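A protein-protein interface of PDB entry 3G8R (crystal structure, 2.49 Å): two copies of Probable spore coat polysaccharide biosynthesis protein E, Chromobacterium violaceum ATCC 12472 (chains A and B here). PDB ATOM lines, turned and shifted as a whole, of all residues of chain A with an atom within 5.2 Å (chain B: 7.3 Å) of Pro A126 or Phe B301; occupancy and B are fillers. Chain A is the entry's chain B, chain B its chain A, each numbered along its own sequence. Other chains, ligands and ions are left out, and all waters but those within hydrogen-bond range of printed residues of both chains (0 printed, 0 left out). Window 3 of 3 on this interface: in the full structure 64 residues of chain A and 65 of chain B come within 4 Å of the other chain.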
ATOM      1  N   THR A  52       0.003  -6.492 -24.022  1.00  0.00           N
ATOM      2  CA  THR A  52       0.613  -5.463 -24.816  1.00  0.00           C
ATOM      3  C   THR A  52       1.616  -4.618 -24.006  1.00  0.00           C
ATOM      4  O   THR A  52       2.576  -4.080 -24.559  1.00  0.00           O
ATOM      5  CB  THR A  52      -0.532  -4.627 -25.432  1.00  0.00           C
ATOM      6  OG1 THR A  52      -0.669  -4.947 -26.829  1.00  0.00           O
ATOM      7  CG2 THR A  52      -0.360  -3.139 -25.245  1.00  0.00           C
ATOM      8  N   GLU A 101      -2.835   3.235 -23.374  1.00  0.00           N
ATOM      9  CA  GLU A 101      -4.035   3.889 -23.877  1.00  0.00           C
ATOM     10  C   GLU A 101      -5.274   2.969 -23.943  1.00  0.00           C
ATOM     11  O   GLU A 101      -6.427   3.405 -23.772  1.00  0.00           O
ATOM     12  CB  GLU A 101      -3.752   4.716 -25.135  1.00  0.00           C
ATOM     13  CG  GLU A 101      -2.620   4.238 -25.975  1.00  0.00           C
ATOM     14  CD  GLU A 101      -1.274   4.637 -25.461  1.00  0.00           C
ATOM     15  OE1 GLU A 101      -0.957   5.838 -25.452  1.00  0.00           O
ATOM     16  OE2 GLU A 101      -0.506   3.723 -25.116  1.00  0.00           O
ATOM     17  N   ASP A 124       4.233  10.995 -19.887  1.00  0.00           N
ATOM     18  CA  ASP A 124       3.989  10.040 -20.960  1.00  0.00           C
ATOM     19  C   ASP A 124       3.011  10.653 -21.955  1.00  0.00           C
ATOM     20  O   ASP A 124       1.815  10.333 -21.961  1.00  0.00           O
ATOM     21  CB  ASP A 124       3.430   8.744 -20.404  1.00  0.00           C
ATOM     22  CG  ASP A 124       3.495   7.593 -21.400  1.00  0.00           C
ATOM     23  OD1 ASP A 124       2.808   7.595 -22.432  1.00  0.00           O
ATOM     24  OD2 ASP A 124       4.259   6.651 -21.127  1.00  0.00           O
ATOM     25  N   TRP A 125       3.522  11.544 -22.798  1.00  0.00           N
ATOM     26  CA  TRP A 125       2.689  12.350 -23.658  1.00  0.00           C
ATOM     27  C   TRP A 125       1.666  11.515 -24.431  1.00  0.00           C
ATOM     28  O   TRP A 125       0.495  11.908 -24.545  1.00  0.00           O
ATOM     29  CB  TRP A 125       3.562  13.235 -24.549  1.00  0.00           C
ATOM     30  CG  TRP A 125       4.201  14.257 -23.698  1.00  0.00           C
ATOM     31  CD1 TRP A 125       5.522  14.306 -23.271  1.00  0.00           C
ATOM     32  CD2 TRP A 125       3.530  15.344 -23.048  1.00  0.00           C
ATOM     33  NE1 TRP A 125       5.694  15.392 -22.411  1.00  0.00           N
ATOM     34  CE2 TRP A 125       4.493  16.037 -22.271  1.00  0.00           C
ATOM     35  CE3 TRP A 125       2.199  15.810 -23.062  1.00  0.00           C
ATOM     36  CZ2 TRP A 125       4.175  17.170 -21.536  1.00  0.00           C
ATOM     37  CZ3 TRP A 125       1.869  16.950 -22.304  1.00  0.00           C
ATOM     38  CH2 TRP A 125       2.862  17.609 -21.551  1.00  0.00           C
ATOM     39  N   PRO A 126       2.077  10.337 -24.935  1.00  0.00           N
ATOM     40  CA  PRO A 126       1.064   9.659 -25.708  1.00  0.00           C
ATOM     41  C   PRO A 126      -0.078   9.234 -24.820  1.00  0.00           C
ATOM     42  O   PRO A 126      -1.218   9.326 -25.259  1.00  0.00           O
ATOM     43  CB  PRO A 126       1.806   8.454 -26.271  1.00  0.00           C
ATOM     44  CG  PRO A 126       3.234   8.901 -26.305  1.00  0.00           C
ATOM     45  CD  PRO A 126       3.374   9.642 -25.028  1.00  0.00           C
ATOM     46  N   LEU A 127       0.214   8.809 -23.591  1.00  0.00           N
ATOM     47  CA  LEU A 127      -0.824   8.458 -22.648  1.00  0.00           C
ATOM     48  C   LEU A 127      -1.599   9.708 -22.268  1.00  0.00           C
ATOM     49  O   LEU A 127      -2.852   9.725 -22.297  1.00  0.00           O
ATOM     50  CB  LEU A 127      -0.233   7.790 -21.407  1.00  0.00           C
ATOM     51  CG  LEU A 127      -1.192   7.424 -20.266  1.00  0.00           C
ATOM     52  CD1 LEU A 127      -2.199   6.420 -20.687  1.00  0.00           C
ATOM     53  CD2 LEU A 127      -0.406   6.901 -19.126  1.00  0.00           C
ATOM     54  N   LEU A 128      -0.857  10.768 -21.956  1.00  0.00           N
ATOM     55  CA  LEU A 128      -1.488  12.042 -21.642  1.00  0.00           C
ATOM     56  C   LEU A 128      -2.494  12.468 -22.685  1.00  0.00           C
ATOM     57  O   LEU A 128      -3.542  13.018 -22.351  1.00  0.00           O
ATOM     58  CB  LEU A 128      -0.466  13.143 -21.522  1.00  0.00           C
ATOM     59  CG  LEU A 128       0.549  13.080 -20.400  1.00  0.00           C
ATOM     60  CD1 LEU A 128       1.185  14.449 -20.301  1.00  0.00           C
ATOM     61  CD2 LEU A 128      -0.054  12.670 -19.057  1.00  0.00           C
ATOM     62  N   GLU A 129      -2.178  12.236 -23.952  1.00  0.00           N
ATOM     63  CA  GLU A 129      -2.986  12.800 -24.996  1.00  0.00           C
ATOM     64  C   GLU A 129      -4.247  11.969 -25.100  1.00  0.00           C
ATOM     65  O   GLU A 129      -5.304  12.432 -25.533  1.00  0.00           O
ATOM     66  CB  GLU A 129      -2.214  12.804 -26.303  1.00  0.00           C
ATOM     67  CG  GLU A 129      -2.442  14.047 -27.125  1.00  0.00           C
ATOM     68  CD  GLU A 129      -1.127  14.665 -27.577  1.00  0.00           C
ATOM     69  OE1 GLU A 129      -0.055  14.039 -27.311  1.00  0.00           O
ATOM     70  OE2 GLU A 129      -1.167  15.775 -28.177  1.00  0.00           O
ATOM     71  N   ARG A 130      -4.125  10.725 -24.664  1.00  0.00           N
ATOM     72  CA  ARG A 130      -5.271   9.861 -24.613  1.00  0.00           C
ATOM     73  C   ARG A 130      -6.120  10.254 -23.438  1.00  0.00           C
ATOM     74  O   ARG A 130      -7.332  10.410 -23.557  1.00  0.00           O
ATOM     75  CB  ARG A 130      -4.845   8.429 -24.456  1.00  0.00           C
ATOM     76  CG  ARG A 130      -6.040   7.515 -24.354  1.00  0.00           C
ATOM     77  CD  ARG A 130      -6.947   7.635 -25.580  1.00  0.00           C
ATOM     78  NE  ARG A 130      -8.148   6.859 -25.329  1.00  0.00           N
ATOM     79  CZ  ARG A 130      -9.153   7.284 -24.577  1.00  0.00           C
ATOM     80  NH1 ARG A 130     -10.191   6.495 -24.353  1.00  0.00           N
ATOM     81  NH2 ARG A 130      -9.101   8.498 -24.031  1.00  0.00           N
ATOM     82  N   ARG B 280       7.446   3.289 -20.029  1.00  0.00           N
ATOM     83  CA  ARG B 280       7.132   2.607 -21.267  1.00  0.00           C
ATOM     84  C   ARG B 280       8.231   2.925 -22.290  1.00  0.00           C
ATOM     85  O   ARG B 280       8.485   4.091 -22.600  1.00  0.00           O
ATOM     86  CB  ARG B 280       5.785   3.118 -21.740  1.00  0.00           C
ATOM     87  CG  ARG B 280       4.759   2.064 -21.960  1.00  0.00           C
ATOM     88  CD  ARG B 280       3.339   2.553 -21.743  1.00  0.00           C
ATOM     89  NE  ARG B 280       3.092   3.896 -22.269  1.00  0.00           N
ATOM     90  CZ  ARG B 280       2.155   4.180 -23.157  1.00  0.00           C
ATOM     91  NH1 ARG B 280       1.399   3.215 -23.614  1.00  0.00           N
ATOM     92  NH2 ARG B 280       1.973   5.417 -23.588  1.00  0.00           N
ATOM     93  N   GLY B 281       8.907   1.900 -22.797  1.00  0.00           N
ATOM     94  CA  GLY B 281       9.959   2.099 -23.786  1.00  0.00           C
ATOM     95  C   GLY B 281       9.361   2.089 -25.177  1.00  0.00           C
ATOM     96  O   GLY B 281       8.242   1.616 -25.372  1.00  0.00           O
ATOM     97  N   VAL B 282      10.111   2.601 -26.147  1.00  0.00           N
ATOM     98  CA  VAL B 282       9.641   2.682 -27.504  1.00  0.00           C
ATOM     99  C   VAL B 282      10.319   1.588 -28.276  1.00  0.00           C
ATOM    100  O   VAL B 282      11.555   1.530 -28.318  1.00  0.00           O
ATOM    101  CB  VAL B 282      10.022   4.018 -28.121  1.00  0.00           C
ATOM    102  CG1 VAL B 282       9.534   4.105 -29.567  1.00  0.00           C
ATOM    103  CG2 VAL B 282       9.460   5.092 -27.334  1.00  0.00           C
ATOM    104  N   PHE B 283       9.517   0.732 -28.904  1.00  0.00           N
ATOM    105  CA  PHE B 283      10.045  -0.386 -29.684  1.00  0.00           C
ATOM    106  C   PHE B 283       9.663  -0.245 -31.132  1.00  0.00           C
ATOM    107  O   PHE B 283       8.577   0.249 -31.436  1.00  0.00           O
ATOM    108  CB  PHE B 283       9.483  -1.721 -29.176  1.00  0.00           C
ATOM    109  CG  PHE B 283       9.947  -2.099 -27.793  1.00  0.00           C
ATOM    110  CD1 PHE B 283      10.986  -3.002 -27.622  1.00  0.00           C
ATOM    111  CD2 PHE B 283       9.343  -1.545 -26.655  1.00  0.00           C
ATOM    112  CE1 PHE B 283      11.413  -3.370 -26.331  1.00  0.00           C
ATOM    113  CE2 PHE B 283       9.757  -1.901 -25.358  1.00  0.00           C
ATOM    114  CZ  PHE B 283      10.790  -2.821 -25.194  1.00  0.00           C
ATOM    115  N   THR B 285       8.177  -1.805 -34.459  1.00  0.00           N
ATOM    116  CA  THR B 285       7.212  -2.866 -34.718  1.00  0.00           C
ATOM    117  C   THR B 285       7.501  -3.566 -36.057  1.00  0.00           C
ATOM    118  O   THR B 285       6.868  -4.575 -36.394  1.00  0.00           O
ATOM    119  CB  THR B 285       5.776  -2.337 -34.713  1.00  0.00           C
ATOM    120  OG1 THR B 285       5.627  -1.387 -35.748  1.00  0.00           O
ATOM    121  CG2 THR B 285       5.480  -1.646 -33.440  1.00  0.00           C
ATOM    122  N   THR B 295       7.594   6.592 -36.979  1.00  0.00           N
ATOM    123  CA  THR B 295       6.185   7.028 -36.919  1.00  0.00           C
ATOM    124  C   THR B 295       5.266   6.147 -36.036  1.00  0.00           C
ATOM    125  O   THR B 295       5.703   5.157 -35.430  1.00  0.00           O
ATOM    126  CB  THR B 295       5.591   7.209 -38.338  1.00  0.00           C
ATOM    127  OG1 THR B 295       5.563   5.943 -39.009  1.00  0.00           O
ATOM    128  CG2 THR B 295       6.428   8.175 -39.177  1.00  0.00           C
ATOM    129  N   ALA B 296       3.995   6.518 -35.957  1.00  0.00           N
ATOM    130  CA  ALA B 296       2.996   5.725 -35.214  1.00  0.00           C
ATOM    131  C   ALA B 296       2.872   4.271 -35.718  1.00  0.00           C
ATOM    132  O   ALA B 296       2.610   3.356 -34.933  1.00  0.00           O
ATOM    133  CB  ALA B 296       1.621   6.430 -35.202  1.00  0.00           C
ATOM    134  N   VAL B 299       6.663   2.117 -34.714  1.00  0.00           N
ATOM    135  CA  VAL B 299       6.936   1.994 -33.269  1.00  0.00           C
ATOM    136  C   VAL B 299       5.703   1.666 -32.432  1.00  0.00           C
ATOM    137  O   VAL B 299       4.584   1.966 -32.816  1.00  0.00           O
ATOM    138  CB  VAL B 299       7.452   3.275 -32.626  1.00  0.00           C
ATOM    139  CG1 VAL B 299       8.615   3.849 -33.371  1.00  0.00           C
ATOM    140  CG2 VAL B 299       6.310   4.280 -32.513  1.00  0.00           C
ATOM    141  N   SER B 300       5.946   1.105 -31.252  1.00  0.00           N
ATOM    142  CA  SER B 300       4.936   0.888 -30.241  1.00  0.00           C
ATOM    143  C   SER B 300       5.537   1.108 -28.843  1.00  0.00           C
ATOM    144  O   SER B 300       6.745   1.146 -28.661  1.00  0.00           O
ATOM    145  CB  SER B 300       4.362  -0.528 -30.368  1.00  0.00           C
ATOM    146  OG  SER B 300       5.278  -1.522 -29.910  1.00  0.00           O
ATOM    147  N   PHE B 301       4.683   1.242 -27.848  1.00  0.00           N
ATOM    148  CA  PHE B 301       5.173   1.492 -26.513  1.00  0.00           C
ATOM    149  C   PHE B 301       4.896   0.299 -25.647  1.00  0.00           C
ATOM    150  O   PHE B 301       3.845  -0.307 -25.750  1.00  0.00           O
ATOM    151  CB  PHE B 301       4.516   2.738 -25.928  1.00  0.00           C
ATOM    152  CG  PHE B 301       4.521   3.886 -26.855  1.00  0.00           C
ATOM    153  CD1 PHE B 301       5.722   4.444 -27.287  1.00  0.00           C
ATOM    154  CD2 PHE B 301       3.349   4.376 -27.360  1.00  0.00           C
ATOM    155  CE1 PHE B 301       5.737   5.499 -28.171  1.00  0.00           C
ATOM    156  CE2 PHE B 301       3.359   5.409 -28.250  1.00  0.00           C
ATOM    157  CZ  PHE B 301       4.551   5.982 -28.647  1.00  0.00           C
ATOM    158  N   ALA B 302       5.822  -0.017 -24.763  1.00  0.00           N
ATOM    159  CA  ALA B 302       5.705  -1.201 -23.954  1.00  0.00           C
ATOM    160  C   ALA B 302       6.771  -1.102 -22.927  1.00  0.00           C
ATOM    161  O   ALA B 302       7.753  -0.406 -23.128  1.00  0.00           O
ATOM    162  CB  ALA B 302       5.909  -2.411 -24.801  1.00  0.00           C
ATOM    163  N   PHE B 303       6.590  -1.801 -21.828  1.00  0.00           N
ATOM    164  CA  PHE B 303       7.546  -1.764 -20.753  1.00  0.00           C
ATOM    165  C   PHE B 303       8.189  -3.118 -20.499  1.00  0.00           C
ATOM    166  O   PHE B 303       7.601  -4.157 -20.847  1.00  0.00           O
ATOM    167  CB  PHE B 303       6.809  -1.269 -19.527  1.00  0.00           C
ATOM    168  CG  PHE B 303       6.927  -2.140 -18.320  1.00  0.00           C
ATOM    169  CD1 PHE B 303       7.468  -1.623 -17.138  1.00  0.00           C
ATOM    170  CD2 PHE B 303       6.421  -3.436 -18.317  1.00  0.00           C
ATOM    171  CE1 PHE B 303       7.575  -2.419 -15.959  1.00  0.00           C
ATOM    172  CE2 PHE B 303       6.501  -4.255 -17.141  1.00  0.00           C
ATOM    173  CZ  PHE B 303       7.086  -3.731 -15.962  1.00  0.00           C
ATOM    174  N   LEU B 310      14.862   4.664 -25.932  1.00  0.00           N
ATOM    175  CA  LEU B 310      14.030   5.828 -25.967  1.00  0.00           C
ATOM    176  C   LEU B 310      12.743   5.381 -25.274  1.00  0.00           C
ATOM    177  O   LEU B 310      12.287   4.249 -25.472  1.00  0.00           O
ATOM    178  CB  LEU B 310      13.784   6.235 -27.418  1.00  0.00           C
ATOM    179  CG  LEU B 310      12.777   7.370 -27.615  1.00  0.00           C
ATOM    180  CD1 LEU B 310      13.495   8.666 -27.557  1.00  0.00           C
ATOM    181  CD2 LEU B 310      12.009   7.262 -28.907  1.00  0.00           C
ATOM    182  N   THR B 311      12.202   6.252 -24.425  1.00  0.00           N
ATOM    183  CA  THR B 311      10.964   5.997 -23.682  1.00  0.00           C
ATOM    184  C   THR B 311       9.836   6.859 -24.209  1.00  0.00           C
ATOM    185  O   THR B 311      10.065   7.850 -24.888  1.00  0.00           O
ATOM    186  CB  THR B 311      11.122   6.313 -22.194  1.00  0.00           C
ATOM    187  OG1 THR B 311      11.003   7.719 -21.993  1.00  0.00           O
ATOM    188  CG2 THR B 311      12.469   5.888 -21.712  1.00  0.00           C
ATOM    189  N   ALA B 312       8.617   6.484 -23.851  1.00  0.00           N
ATOM    190  CA  ALA B 312       7.405   7.119 -24.329  1.00  0.00           C
ATOM    191  C   ALA B 312       7.351   8.531 -23.816  1.00  0.00           C
ATOM    192  O   ALA B 312       6.834   9.435 -24.488  1.00  0.00           O
ATOM    193  CB  ALA B 312       6.208   6.347 -23.850  1.00  0.00           C
ATOM    194  N   ASN B 313       7.913   8.722 -22.630  1.00  0.00           N
ATOM    195  CA  ASN B 313       8.077  10.047 -22.069  1.00  0.00           C
ATOM    196  C   ASN B 313       8.849  11.033 -22.943  1.00  0.00           C
ATOM    197  O   ASN B 313       9.022  12.185 -22.569  1.00  0.00           O
ATOM    198  CB  ASN B 313       8.701   9.931 -20.696  1.00  0.00           C
ATOM    199  CG  ASN B 313       7.836   9.138 -19.755  1.00  0.00           C
ATOM    200  OD1 ASN B 313       7.532   7.957 -20.008  1.00  0.00           O
ATOM    201  ND2 ASN B 313       7.405   9.779 -18.669  1.00  0.00           N
ATOM    202  N   GLU B 314       9.313  10.568 -24.103  1.00  0.00           N
ATOM    203  CA  GLU B 314      10.114  11.383 -25.009  1.00  0.00           C
ATOM    204  C   GLU B 314       9.521  11.383 -26.418  1.00  0.00           C
ATOM    205  O   GLU B 314      10.078  12.002 -27.328  1.00  0.00           O
ATOM    206  CB  GLU B 314      11.562  10.903 -25.035  1.00  0.00           C
ATOM    207  CG  GLU B 314      12.189  10.755 -23.662  1.00  0.00           C
ATOM    208  CD  GLU B 314      13.456   9.891 -23.681  1.00  0.00           C
ATOM    209  OE1 GLU B 314      14.523  10.456 -24.024  1.00  0.00           O
ATOM    210  OE2 GLU B 314      13.400   8.664 -23.365  1.00  0.00           O
ATOM    211  N   TRP B 315       8.391  10.694 -26.580  1.00  0.00           N
ATOM    212  CA  TRP B 315       7.743  10.550 -27.879  1.00  0.00           C
ATOM    213  C   TRP B 315       6.910  11.767 -28.119  1.00  0.00           C
ATOM    214  O   TRP B 315       6.674  12.498 -27.180  1.00  0.00           O
ATOM    215  CB  TRP B 315       6.872   9.307 -27.928  1.00  0.00           C
ATOM    216  CG  TRP B 315       6.404   9.002 -29.305  1.00  0.00           C
ATOM    217  CD1 TRP B 315       5.117   9.067 -29.767  1.00  0.00           C
ATOM    218  CD2 TRP B 315       7.207   8.612 -30.416  1.00  0.00           C
ATOM    219  NE1 TRP B 315       5.063   8.732 -31.095  1.00  0.00           N
ATOM    220  CE2 TRP B 315       6.334   8.440 -31.520  1.00  0.00           C
ATOM    221  CE3 TRP B 315       8.588   8.386 -30.593  1.00  0.00           C
ATOM    222  CZ2 TRP B 315       6.789   8.056 -32.778  1.00  0.00           C
ATOM    223  CZ3 TRP B 315       9.046   8.016 -31.841  1.00  0.00           C
ATOM    224  CH2 TRP B 315       8.145   7.842 -32.918  1.00  0.00           C
ATOM    225  N   SER B 316       6.474  12.003 -29.358  1.00  0.00           N
ATOM    226  CA  SER B 316       5.825  13.258 -29.670  1.00  0.00           C
ATOM    227  C   SER B 316       4.628  13.278 -30.621  1.00  0.00           C
ATOM    228  O   SER B 316       3.885  14.257 -30.621  1.00  0.00           O
ATOM    229  CB  SER B 316       6.861  14.289 -30.110  1.00  0.00           C
ATOM    230  OG  SER B 316       6.362  15.147 -31.135  1.00  0.00           O
ATOM    231  N   LYS B 317       4.396  12.260 -31.436  1.00  0.00           N
ATOM    232  CA  LYS B 317       3.182  12.304 -32.317  1.00  0.00           C
ATOM    233  C   LYS B 317       3.361  13.092 -33.602  1.00  0.00           C
ATOM    234  O   LYS B 317       2.780  12.725 -34.633  1.00  0.00           O
ATOM    235  CB  LYS B 317       1.939  12.797 -31.568  1.00  0.00           C
ATOM    236  CG  LYS B 317       0.965  13.637 -32.357  1.00  0.00           C
ATOM    237  CD  LYS B 317       0.067  14.362 -31.375  1.00  0.00           C
ATOM    238  CE  LYS B 317      -0.482  15.621 -31.935  1.00  0.00           C
ATOM    239  NZ  LYS B 317      -1.109  16.331 -30.808  1.00  0.00           N
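Among the printed residues, pairs that only touch across the chains: Thr A52 with Ala B302, Asp A124 with Ala B312, Asp A124 with Asn B313, Pro A126 with Phe B301, Pro A126 with Ala B312, Pro A126 with Trp B315 and Leu A127 with Arg B280.
No position is printed for both chains.
Of the 10 pairs that touch across the chains among the printed residues, none has its exchanged pair printed and touching as well.
The side-chain hydroxyl (OG1) of Thr B311 sits close to the backbone NH (N) of Asn B313, 3.3 Å away.
OD1 of Asp A124 is in hydrogen-bond range of N of Leu A127 (3.1 Å).
The backbone NH (N) of Gly B281 lies within hydrogen-bond range of the backbone carbonyl oxygen (O) of Ala B302 (2.6 Å).
N of Ala B312 is in hydrogen-bond range of O of Arg B280 (2.7 Å).
OD1 of Asp A124 is in salt-bridge range of NH2 of Arg B280 (2.6 Å).
The side-chain amino group of Lys B317 is in salt-bridge range of the side-chain carboxylate of Glu A129 (2.7 Å).
The side-chain carboxylate of Glu A101 is in salt-bridge range of the guanidinium group of Arg B280.
Of the 9 printed residues of chain A, 6 touch a printed residue of chain B.
Hydrophobic or aromatic side chains of chain A that line the printed part of chain B: Pro A126 and Leu A127.
Printed residues of chain B that touch a printed residue of chain A: Arg B280, Phe B301, Ala B302, Ala B312, Asn B313, Trp B315 and Lys B317.
Hydrophobic or aromatic side chains of chain B that line the printed part of chain A: Phe B301, Ala B302, Ala B312 and Trp B315.
Along chain B the printed residues that touch a printed residue of chain A span positions 280 to 317.
Among the printed residues, 10 pairs touch across the chains.
Of the printed residues of chain B, Leu A127 touches Arg B280 (3.8 Å).
Of the printed residues of chain B, Glu A129 touches Lys B317 (2.7 Å).
Arg A130 touches none of the printed residues of chain B.
Of chain A, only Pro A126 comes within 4 Å of Phe B301.
Of the printed residues of chain A, Asn B313 touches Asp A124 (3.6 Å).
Printed residues of chain A within 4 Å of Lys B317: Glu A129.
The nearest printed residue of chain B that does not touch Leu A127 is Ala B312 (6.5 Å).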
